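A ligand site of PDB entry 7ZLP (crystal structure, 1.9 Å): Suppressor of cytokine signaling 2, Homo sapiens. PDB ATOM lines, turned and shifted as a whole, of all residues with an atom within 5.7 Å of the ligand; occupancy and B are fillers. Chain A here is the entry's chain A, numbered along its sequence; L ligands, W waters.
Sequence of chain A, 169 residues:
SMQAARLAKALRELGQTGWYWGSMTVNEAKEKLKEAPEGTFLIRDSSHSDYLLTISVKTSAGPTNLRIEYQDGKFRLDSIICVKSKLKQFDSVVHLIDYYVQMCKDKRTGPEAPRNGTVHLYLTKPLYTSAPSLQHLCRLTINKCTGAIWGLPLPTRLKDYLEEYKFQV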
ATOM      1  N   MET A  24     -14.697  -3.203   8.749  1.00  0.00           N
ATOM      2  CA  MET A  24     -15.352  -4.367   8.187  1.00  0.00           C
ATOM      3  C   MET A  24     -16.532  -4.683   9.080  1.00  0.00           C
ATOM      4  O   MET A  24     -16.352  -4.818  10.297  1.00  0.00           O
ATOM      5  CB  MET A  24     -14.373  -5.546   8.091  1.00  0.00           C
ATOM      6  CG  MET A  24     -15.006  -6.891   7.736  1.00  0.00           C
ATOM      7  SD  MET A  24     -13.795  -8.230   7.715  1.00  0.00           S
ATOM      8  CE  MET A  24     -14.131  -8.926   6.090  1.00  0.00           C
ATOM      9  N   VAL A  26     -19.845  -6.696  10.759  1.00  0.00           N
ATOM     10  CA  VAL A  26     -20.000  -8.063  11.252  1.00  0.00           C
ATOM     11  C   VAL A  26     -20.569  -8.941  10.143  1.00  0.00           C
ATOM     12  O   VAL A  26     -20.187 -10.116  10.022  1.00  0.00           O
ATOM     13  CB  VAL A  26     -20.884  -8.068  12.527  1.00  0.00           C
ATOM     14  CG1 VAL A  26     -22.259  -7.493  12.260  1.00  0.00           C
ATOM     15  CG2 VAL A  26     -21.004  -9.468  13.104  1.00  0.00           C
ATOM     16  N   ASN A  27     -21.426  -8.384   9.298  1.00  0.00           N
ATOM     17  CA  ASN A  27     -22.001  -9.139   8.188  1.00  0.00           C
ATOM     18  C   ASN A  27     -20.988  -9.375   7.075  1.00  0.00           C
ATOM     19  O   ASN A  27     -21.018 -10.410   6.404  1.00  0.00           O
ATOM     20  CB  ASN A  27     -23.225  -8.436   7.624  1.00  0.00           C
ATOM     21  CG  ASN A  27     -24.489  -8.662   8.448  1.00  0.00           C
ATOM     22  OD1 ASN A  27     -24.756  -9.783   8.900  1.00  0.00           O
ATOM     23  ND2 ASN A  27     -25.314  -7.623   8.581  1.00  0.00           N
ATOM     24  N   LYS A  30     -18.878 -12.180   8.391  1.00  0.00           N
ATOM     25  CA  LYS A  30     -19.646 -13.406   8.246  1.00  0.00           C
ATOM     26  C   LYS A  30     -19.525 -13.966   6.831  1.00  0.00           C
ATOM     27  O   LYS A  30     -19.284 -15.167   6.646  1.00  0.00           O
ATOM     28  CB  LYS A  30     -21.113 -13.136   8.595  1.00  0.00           C
ATOM     29  CG  LYS A  30     -22.043 -14.360   8.487  1.00  0.00           C
ATOM     30  CD  LYS A  30     -23.503 -13.950   8.641  1.00  0.00           C
ATOM     31  CE  LYS A  30     -23.888 -12.936   7.584  1.00  0.00           C
ATOM     32  NZ  LYS A  30     -25.328 -12.561   7.643  1.00  0.00           N
ATOM     33  N   ARG A  44     -10.669  -7.156  13.064  1.00  0.00           N
ATOM     34  CA  ARG A  44     -11.269  -6.013  12.402  1.00  0.00           C
ATOM     35  C   ARG A  44     -11.651  -5.017  13.485  1.00  0.00           C
ATOM     36  O   ARG A  44     -11.675  -5.338  14.667  1.00  0.00           O
ATOM     37  CB  ARG A  44     -12.495  -6.416  11.578  1.00  0.00           C
ATOM     38  CG  ARG A  44     -13.613  -7.017  12.420  1.00  0.00           C
ATOM     39  CD  ARG A  44     -14.852  -7.412  11.570  1.00  0.00           C
ATOM     40  NE  ARG A  44     -15.818  -8.131  12.394  1.00  0.00           N
ATOM     41  CZ  ARG A  44     -16.673  -7.531  13.215  1.00  0.00           C
ATOM     42  NH1 ARG A  44     -16.755  -6.198  13.298  1.00  0.00           N
ATOM     43  NH2 ARG A  44     -17.489  -8.283  13.964  1.00  0.00           N
ATOM     44  N   ASP A  45     -11.944  -3.796  13.053  1.00  0.00           N
ATOM     45  CA  ASP A  45     -12.458  -2.781  13.955  1.00  0.00           C
ATOM     46  C   ASP A  45     -13.829  -3.198  14.462  1.00  0.00           C
ATOM     47  O   ASP A  45     -14.662  -3.686  13.701  1.00  0.00           O
ATOM     48  CB  ASP A  45     -12.591  -1.423  13.255  1.00  0.00           C
ATOM     49  CG  ASP A  45     -11.261  -0.816  12.854  1.00  0.00           C
ATOM     50  OD1 ASP A  45     -10.211  -1.339  13.295  1.00  0.00           O
ATOM     51  OD2 ASP A  45     -11.274   0.180  12.082  1.00  0.00           O
ATOM     52  N   SER A  46     -14.099  -2.942  15.743  1.00  0.00           N
ATOM     53  CA  SER A  46     -15.435  -3.187  16.271  1.00  0.00           C
ATOM     54  C   SER A  46     -16.383  -2.073  15.869  1.00  0.00           C
ATOM     55  O   SER A  46     -15.995  -0.898  15.741  1.00  0.00           O
ATOM     56  CB  SER A  46     -15.397  -3.304  17.800  1.00  0.00           C
ATOM     57  OG  SER A  46     -16.702  -3.325  18.314  1.00  0.00           O
ATOM     58  N   SER A  47     -17.647  -2.440  15.633  1.00  0.00           N
ATOM     59  CA  SER A  47     -18.691  -1.429  15.452  1.00  0.00           C
ATOM     60  C   SER A  47     -19.168  -0.826  16.756  1.00  0.00           C
ATOM     61  O   SER A  47     -19.955   0.101  16.744  1.00  0.00           O
ATOM     62  CB  SER A  47     -19.920  -2.001  14.747  1.00  0.00           C
ATOM     63  OG  SER A  47     -19.608  -2.438  13.448  1.00  0.00           O
ATOM     64  N   HIS A  48     -18.753  -1.366  17.895  1.00  0.00           N
ATOM     65  CA  HIS A  48     -19.315  -0.939  19.169  1.00  0.00           C
ATOM     66  C   HIS A  48     -18.528   0.265  19.669  1.00  0.00           C
ATOM     67  O   HIS A  48     -17.294   0.251  19.650  1.00  0.00           O
ATOM     68  CB  HIS A  48     -19.278  -2.081  20.189  1.00  0.00           C
ATOM     69  CG  HIS A  48     -20.031  -1.801  21.446  1.00  0.00           C
ATOM     70  ND1 HIS A  48     -19.607  -0.855  22.361  1.00  0.00           N
ATOM     71  CD2 HIS A  48     -21.165  -2.335  21.953  1.00  0.00           C
ATOM     72  CE1 HIS A  48     -20.457  -0.817  23.370  1.00  0.00           C
ATOM     73  NE2 HIS A  48     -21.404  -1.711  23.148  1.00  0.00           N
ATOM     74  N   TYR A  51     -15.451  -0.372  22.067  1.00  0.00           N
ATOM     75  CA  TYR A  51     -14.379  -1.308  21.722  1.00  0.00           C
ATOM     76  C   TYR A  51     -13.634  -0.901  20.447  1.00  0.00           C
ATOM     77  O   TYR A  51     -14.247  -0.500  19.451  1.00  0.00           O
ATOM     78  CB  TYR A  51     -14.946  -2.733  21.548  1.00  0.00           C
ATOM     79  CG  TYR A  51     -15.595  -3.300  22.799  1.00  0.00           C
ATOM     80  CD1 TYR A  51     -16.866  -2.913  23.198  1.00  0.00           C
ATOM     81  CD2 TYR A  51     -14.914  -4.239  23.567  1.00  0.00           C
ATOM     82  CE1 TYR A  51     -17.451  -3.449  24.351  1.00  0.00           C
ATOM     83  CE2 TYR A  51     -15.495  -4.785  24.712  1.00  0.00           C
ATOM     84  CZ  TYR A  51     -16.749  -4.382  25.103  1.00  0.00           C
ATOM     85  OH  TYR A  51     -17.314  -4.911  26.226  1.00  0.00           O
ATOM     86  N   LEU A  53     -11.516  -3.216  18.761  1.00  0.00           N
ATOM     87  CA  LEU A  53     -11.236  -4.333  17.862  1.00  0.00           C
ATOM     88  C   LEU A  53     -12.086  -5.547  18.213  1.00  0.00           C
ATOM     89  O   LEU A  53     -12.453  -5.767  19.370  1.00  0.00           O
ATOM     90  CB  LEU A  53      -9.745  -4.718  17.902  1.00  0.00           C
ATOM     91  CG  LEU A  53      -8.734  -3.703  17.384  1.00  0.00           C
ATOM     92  CD1 LEU A  53      -7.347  -3.952  18.008  1.00  0.00           C
ATOM     93  CD2 LEU A  53      -8.693  -3.763  15.853  1.00  0.00           C
ATOM     94  N   THR A  54     -12.332  -6.371  17.206  1.00  0.00           N
ATOM     95  CA  THR A  54     -13.134  -7.578  17.335  1.00  0.00           C
ATOM     96  C   THR A  54     -12.485  -8.679  16.525  1.00  0.00           C
ATOM     97  O   THR A  54     -12.088  -8.453  15.386  1.00  0.00           O
ATOM     98  CB  THR A  54     -14.555  -7.342  16.807  1.00  0.00           C
ATOM     99  OG1 THR A  54     -15.213  -6.407  17.645  1.00  0.00           O
ATOM    100  CG2 THR A  54     -15.339  -8.645  16.819  1.00  0.00           C
ATOM    101  N   VAL A  57     -14.105 -15.316  13.824  1.00  0.00           N
ATOM    102  CA  VAL A  57     -13.512 -16.653  13.736  1.00  0.00           C
ATOM    103  C   VAL A  57     -14.572 -17.645  13.269  1.00  0.00           C
ATOM    104  O   VAL A  57     -15.713 -17.621  13.754  1.00  0.00           O
ATOM    105  CB  VAL A  57     -12.870 -17.095  15.068  1.00  0.00           C
ATOM    106  CG1 VAL A  57     -13.856 -16.967  16.240  1.00  0.00           C
ATOM    107  CG2 VAL A  57     -12.300 -18.550  14.994  1.00  0.00           C
ATOM    108  N   PRO A  63     -19.417 -18.517  11.318  1.00  0.00           N
ATOM    109  CA  PRO A  63     -18.554 -17.487  11.896  1.00  0.00           C
ATOM    110  C   PRO A  63     -19.191 -16.917  13.167  1.00  0.00           C
ATOM    111  O   PRO A  63     -20.416 -16.836  13.282  1.00  0.00           O
ATOM    112  CB  PRO A  63     -18.448 -16.430  10.786  1.00  0.00           C
ATOM    113  CG  PRO A  63     -18.936 -17.145   9.504  1.00  0.00           C
ATOM    114  CD  PRO A  63     -19.937 -18.146   9.980  1.00  0.00           C
ATOM    115  N   THR A  64     -18.351 -16.595  14.147  1.00  0.00           N
ATOM    116  CA  THR A  64     -18.771 -15.935  15.365  1.00  0.00           C
ATOM    117  C   THR A  64     -17.807 -14.781  15.638  1.00  0.00           C
ATOM    118  O   THR A  64     -16.797 -14.616  14.948  1.00  0.00           O
ATOM    119  CB  THR A  64     -18.861 -16.926  16.555  1.00  0.00           C
ATOM    120  OG1 THR A  64     -19.613 -16.345  17.641  1.00  0.00           O
ATOM    121  CG2 THR A  64     -17.488 -17.334  17.056  1.00  0.00           C
ATOM    122  N   ASN A  65     -18.127 -13.964  16.635  1.00  0.00           N
ATOM    123  CA  ASN A  65     -17.384 -12.730  16.857  1.00  0.00           C
ATOM    124  C   ASN A  65     -17.077 -12.543  18.330  1.00  0.00           C
ATOM    125  O   ASN A  65     -17.940 -12.774  19.171  1.00  0.00           O
ATOM    126  CB  ASN A  65     -18.157 -11.524  16.358  1.00  0.00           C
ATOM    127  CG  ASN A  65     -18.463 -11.599  14.888  1.00  0.00           C
ATOM    128  OD1 ASN A  65     -17.705 -11.092  14.074  1.00  0.00           O
ATOM    129  ND2 ASN A  65     -19.558 -12.263  14.548  1.00  0.00           N
ATOM    130  N   LEU A  66     -15.852 -12.083  18.643  1.00  0.00           N
ATOM    131  CA  LEU A  66     -15.436 -11.890  20.023  1.00  0.00           C
ATOM    132  C   LEU A  66     -14.678 -10.575  20.125  1.00  0.00           C
ATOM    133  O   LEU A  66     -13.647 -10.393  19.492  1.00  0.00           O
ATOM    134  CB  LEU A  66     -14.536 -13.056  20.488  1.00  0.00           C
ATOM    135  CG  LEU A  66     -14.066 -13.106  21.953  1.00  0.00           C
ATOM    136  CD1 LEU A  66     -15.214 -12.814  22.941  1.00  0.00           C
ATOM    137  CD2 LEU A  66     -13.474 -14.493  22.197  1.00  0.00           C
ATOM    138  N   ARG A  67     -15.203  -9.650  20.921  1.00  0.00           N
ATOM    139  CA  ARG A  67     -14.583  -8.338  21.077  1.00  0.00           C
ATOM    140  C   ARG A  67     -13.321  -8.435  21.922  1.00  0.00           C
ATOM    141  O   ARG A  67     -13.172  -9.324  22.756  1.00  0.00           O
ATOM    142  CB  ARG A  67     -15.589  -7.372  21.714  1.00  0.00           C
ATOM    143  CG  ARG A  67     -16.790  -7.111  20.814  1.00  0.00           C
ATOM    144  CD  ARG A  67     -17.756  -6.115  21.407  1.00  0.00           C
ATOM    145  NE  ARG A  67     -18.851  -5.858  20.477  1.00  0.00           N
ATOM    146  CZ  ARG A  67     -20.127  -5.841  20.827  1.00  0.00           C
ATOM    147  NH1 ARG A  67     -20.506  -5.950  22.090  1.00  0.00           N
ATOM    148  NH2 ARG A  67     -21.052  -5.712  19.876  1.00  0.00           N
ATOM    149  N   ILE A  80     -17.377 -10.051  29.283  1.00  0.00           N
ATOM    150  CA  ILE A  80     -18.712 -10.613  29.453  1.00  0.00           C
ATOM    151  C   ILE A  80     -18.703 -12.117  29.275  1.00  0.00           C
ATOM    152  O   ILE A  80     -19.674 -12.803  29.622  1.00  0.00           O
ATOM    153  CB  ILE A  80     -19.659  -9.871  28.489  1.00  0.00           C
ATOM    154  CG1 ILE A  80     -19.401 -10.251  27.019  1.00  0.00           C
ATOM    155  CG2 ILE A  80     -19.516  -8.355  28.706  1.00  0.00           C
ATOM    156  CD1 ILE A  80     -19.923 -11.621  26.551  1.00  0.00           C
ATOM    157  N   ILE A  81     -17.606 -12.635  28.744  1.00  0.00           N
ATOM    158  CA  ILE A  81     -17.486 -14.037  28.364  1.00  0.00           C
ATOM    159  C   ILE A  81     -17.122 -14.923  29.559  1.00  0.00           C
ATOM    160  O   ILE A  81     -17.599 -16.052  29.692  1.00  0.00           O
ATOM    161  CB  ILE A  81     -16.457 -14.094  27.226  1.00  0.00           C
ATOM    162  CG1 ILE A  81     -17.164 -13.991  25.859  1.00  0.00           C
ATOM    163  CG2 ILE A  81     -15.471 -15.223  27.361  1.00  0.00           C
ATOM    164  N   HIS A 120     -13.005 -20.468  25.885  1.00  0.00           N
ATOM    165  CA  HIS A 120     -13.011 -21.331  24.702  1.00  0.00           C
ATOM    166  C   HIS A 120     -12.752 -20.480  23.460  1.00  0.00           C
ATOM    167  O   HIS A 120     -13.645 -19.736  23.016  1.00  0.00           O
ATOM    168  CB  HIS A 120     -14.326 -22.087  24.565  1.00  0.00           C
ATOM    169  CG  HIS A 120     -14.361 -23.008  23.385  1.00  0.00           C
ATOM    170  ND1 HIS A 120     -13.257 -23.758  23.012  1.00  0.00           N
ATOM    171  CD2 HIS A 120     -15.337 -23.298  22.500  1.00  0.00           C
ATOM    172  CE1 HIS A 120     -13.565 -24.472  21.936  1.00  0.00           C
ATOM    173  NE2 HIS A 120     -14.817 -24.213  21.605  1.00  0.00           N
ATOM    174  N   LEU A 121     -11.564 -20.617  22.880  1.00  0.00           N
ATOM    175  CA  LEU A 121     -11.219 -19.878  21.667  1.00  0.00           C
ATOM    176  C   LEU A 121     -10.329 -20.749  20.800  1.00  0.00           C
ATOM    177  O   LEU A 121      -9.132 -20.920  21.087  1.00  0.00           O
ATOM    178  CB  LEU A 121     -10.522 -18.557  22.002  1.00  0.00           C
ATOM    179  CG  LEU A 121     -10.240 -17.687  20.774  1.00  0.00           C
ATOM    180  CD1 LEU A 121     -11.547 -17.431  20.032  1.00  0.00           C
ATOM    181  CD2 LEU A 121      -9.590 -16.346  21.162  1.00  0.00           C
HETATM  182  C1  LIG L   1     -22.482 -13.951  14.014  1.00  0.00           C
HETATM  183  C2  LIG L   1     -21.392 -13.487  20.531  1.00  0.00           C
HETATM  184  C3  LIG L   1     -20.160 -14.983  22.157  1.00  0.00           C
HETATM  185  C4  LIG L   1     -18.230 -15.907  20.830  1.00  0.00           C
HETATM  186  C5  LIG L   1     -16.878 -16.547  23.175  1.00  0.00           C
HETATM  187  C6  LIG L   1     -18.115 -15.950  23.232  1.00  0.00           C
HETATM  188  C7  LIG L   1     -21.451 -11.044  19.999  1.00  0.00           C
HETATM  189  C8  LIG L   1     -19.573  -9.544  19.240  1.00  0.00           C
HETATM  190  C9  LIG L   1     -19.740  -8.240  17.222  1.00  0.00           C
HETATM  191  C10 LIG L   1     -22.137 -13.358  17.268  1.00  0.00           C
HETATM  192  C11 LIG L   1     -23.313 -13.751  16.381  1.00  0.00           C
HETATM  193  C12 LIG L   1     -23.176 -13.222  14.963  1.00  0.00           C
HETATM  194  C13 LIG L   1     -23.778 -12.015  14.621  1.00  0.00           C
HETATM  195  C14 LIG L   1     -23.676 -11.541  13.329  1.00  0.00           C
HETATM  196  C15 LIG L   1     -22.969 -12.270  12.386  1.00  0.00           C
HETATM  197  C16 LIG L   1     -22.363 -13.463  12.715  1.00  0.00           C
HETATM  198  C17 LIG L   1     -21.306 -12.453  19.434  1.00  0.00           C
HETATM  199  C18 LIG L   1     -18.793 -15.645  22.058  1.00  0.00           C
HETATM  200  C19 LIG L   1     -16.968 -16.501  20.770  1.00  0.00           C
HETATM  201  C20 LIG L   1     -16.299 -16.825  21.950  1.00  0.00           C
HETATM  202  C21 LIG L   1     -20.839 -10.030  19.008  1.00  0.00           C
HETATM  203  C22 LIG L   1     -19.022  -8.641  18.334  1.00  0.00           C
HETATM  204  C23 LIG L   1     -21.016  -8.706  17.009  1.00  0.00           C
HETATM  205  C24 LIG L   1     -21.562  -9.619  17.906  1.00  0.00           C
HETATM  206  F1  LIG L   1     -22.852 -11.798  11.114  1.00  0.00           F
HETATM  207  F2  LIG L   1     -15.054 -17.406  21.944  1.00  0.00           F
HETATM  208  N1  LIG L   1     -22.408 -12.798  18.566  1.00  0.00           N
HETATM  209  N2  LIG L   1     -20.174 -13.989  21.118  1.00  0.00           N
HETATM  210  O1  LIG L   1     -21.008 -13.506  16.918  1.00  0.00           O
HETATM  211  O2  LIG L   1     -22.456 -13.885  20.876  1.00  0.00           O
HETATM  212  O3  LIG L   1     -19.174  -7.343  16.299  1.00  0.00           O
HETATM  213  O4  LIG L   1     -20.235  -5.179  17.139  1.00  0.00           O
HETATM  214  O5  LIG L   1     -18.499  -5.188  15.349  1.00  0.00           O
HETATM  215  O6  LIG L   1     -17.835  -5.709  17.719  1.00  0.00           O
HETATM  216  P1  LIG L   1     -18.933  -5.761  16.657  1.00  0.00           P
HETATM  217  O   HOH W   1     -22.647  -5.800  16.199  1.00  0.00           O
HETATM  218  O   HOH W   2     -19.363 -12.046  11.739  1.00  0.00           O
HETATM  219  O   HOH W   3     -22.097 -16.695  17.588  1.00  0.00           O
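Water W3 bridges the side-chain hydroxyl of Thr 64 (2.5 Å) and an oxygen (O1) of the ligand (3.4 Å).
Water W2 lies within hydrogen-bond range of O of Val 26, ND2 of Asn 65 and N of Lys 30.
An oxygen (O6) of the ligand lies within hydrogen-bond range of the side-chain hydroxyl (OG) of Ser 46 (2.7 Å).
An oxygen (O6) of the ligand sits at hydrogen-bond distance from the side-chain hydroxyl (OG1) of Thr 54 (2.7 Å).
An oxygen (O5) of the ligand lies within salt-bridge range of the guanidinium group (NH1) of Arg 44 (2.9 Å).
N of Ser 47 sits at hydrogen-bond distance from O5 of the ligand (2.9 Å).
The guanidinium group (NH2) of Arg 67 is in salt-bridge range of an oxygen (O4) of the ligand, at 2.9 Å.
N of Asn 65 sits at hydrogen-bond distance from O1 of the ligand, at 2.9 Å.
A nitrogen (N2) of the ligand sits at hydrogen-bond distance from the backbone carbonyl oxygen (O) of Asn 65, 3.2 Å away.
The side-chain amide nitrogen (ND2) of Asn 65 lies within hydrogen-bond range of an oxygen (O1) of the ligand, at 3.0 Å.
An oxygen (O1) of the ligand lies within hydrogen-bond range of the side-chain hydroxyl (OG1) of Thr 64, at 3.2 Å.
The backbone carbonyl oxygen (O) of Val 26 sits close to a fluorine (F1) of the ligand.
O of His 120 sits close to F2 of the ligand.
Residues that only touch the ligand: Leu 66 (3.3 Å), Lys 30 (3.3 Å), Ile 81 (3.4 Å), Asn 27 (3.5 Å), Pro 63 (3.6 Å) and Leu 121 (3.99 Å).
Hydrophobic or aromatic side chains that line the ligand: Val 26, Leu 66, Ile 81 and Leu 121.
Within 4 Å of the ligand: Val 26, Asn 27, Lys 30, Arg 44, Ser 46, Ser 47, Thr 54, Pro 63, Thr 64, Asn 65, Leu 66, Arg 67, Ile 81, His 120 and Leu 121.
OG of Ser 46 lies close to OG1 of Thr 54.
The side-chain hydroxyl of Ser 46 sits at hydrogen-bond distance from the backbone NH of His 48 (2.9 Å).
N of Thr 54 lies within hydrogen-bond range of O of Arg 44, at 2.8 Å.
The guanidinium group (NH2) of Arg 44 lies within hydrogen-bond range of the side-chain amide oxygen (OD1) of Asn 65.
NH1 of Arg 44 sits close to O of Met 24 (3.3 Å).
N of Thr 64 sits at hydrogen-bond distance from O of Val 57.
OD1 of Asn 27 lies within hydrogen-bond range of NZ of Lys 30, at 3.1 Å.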
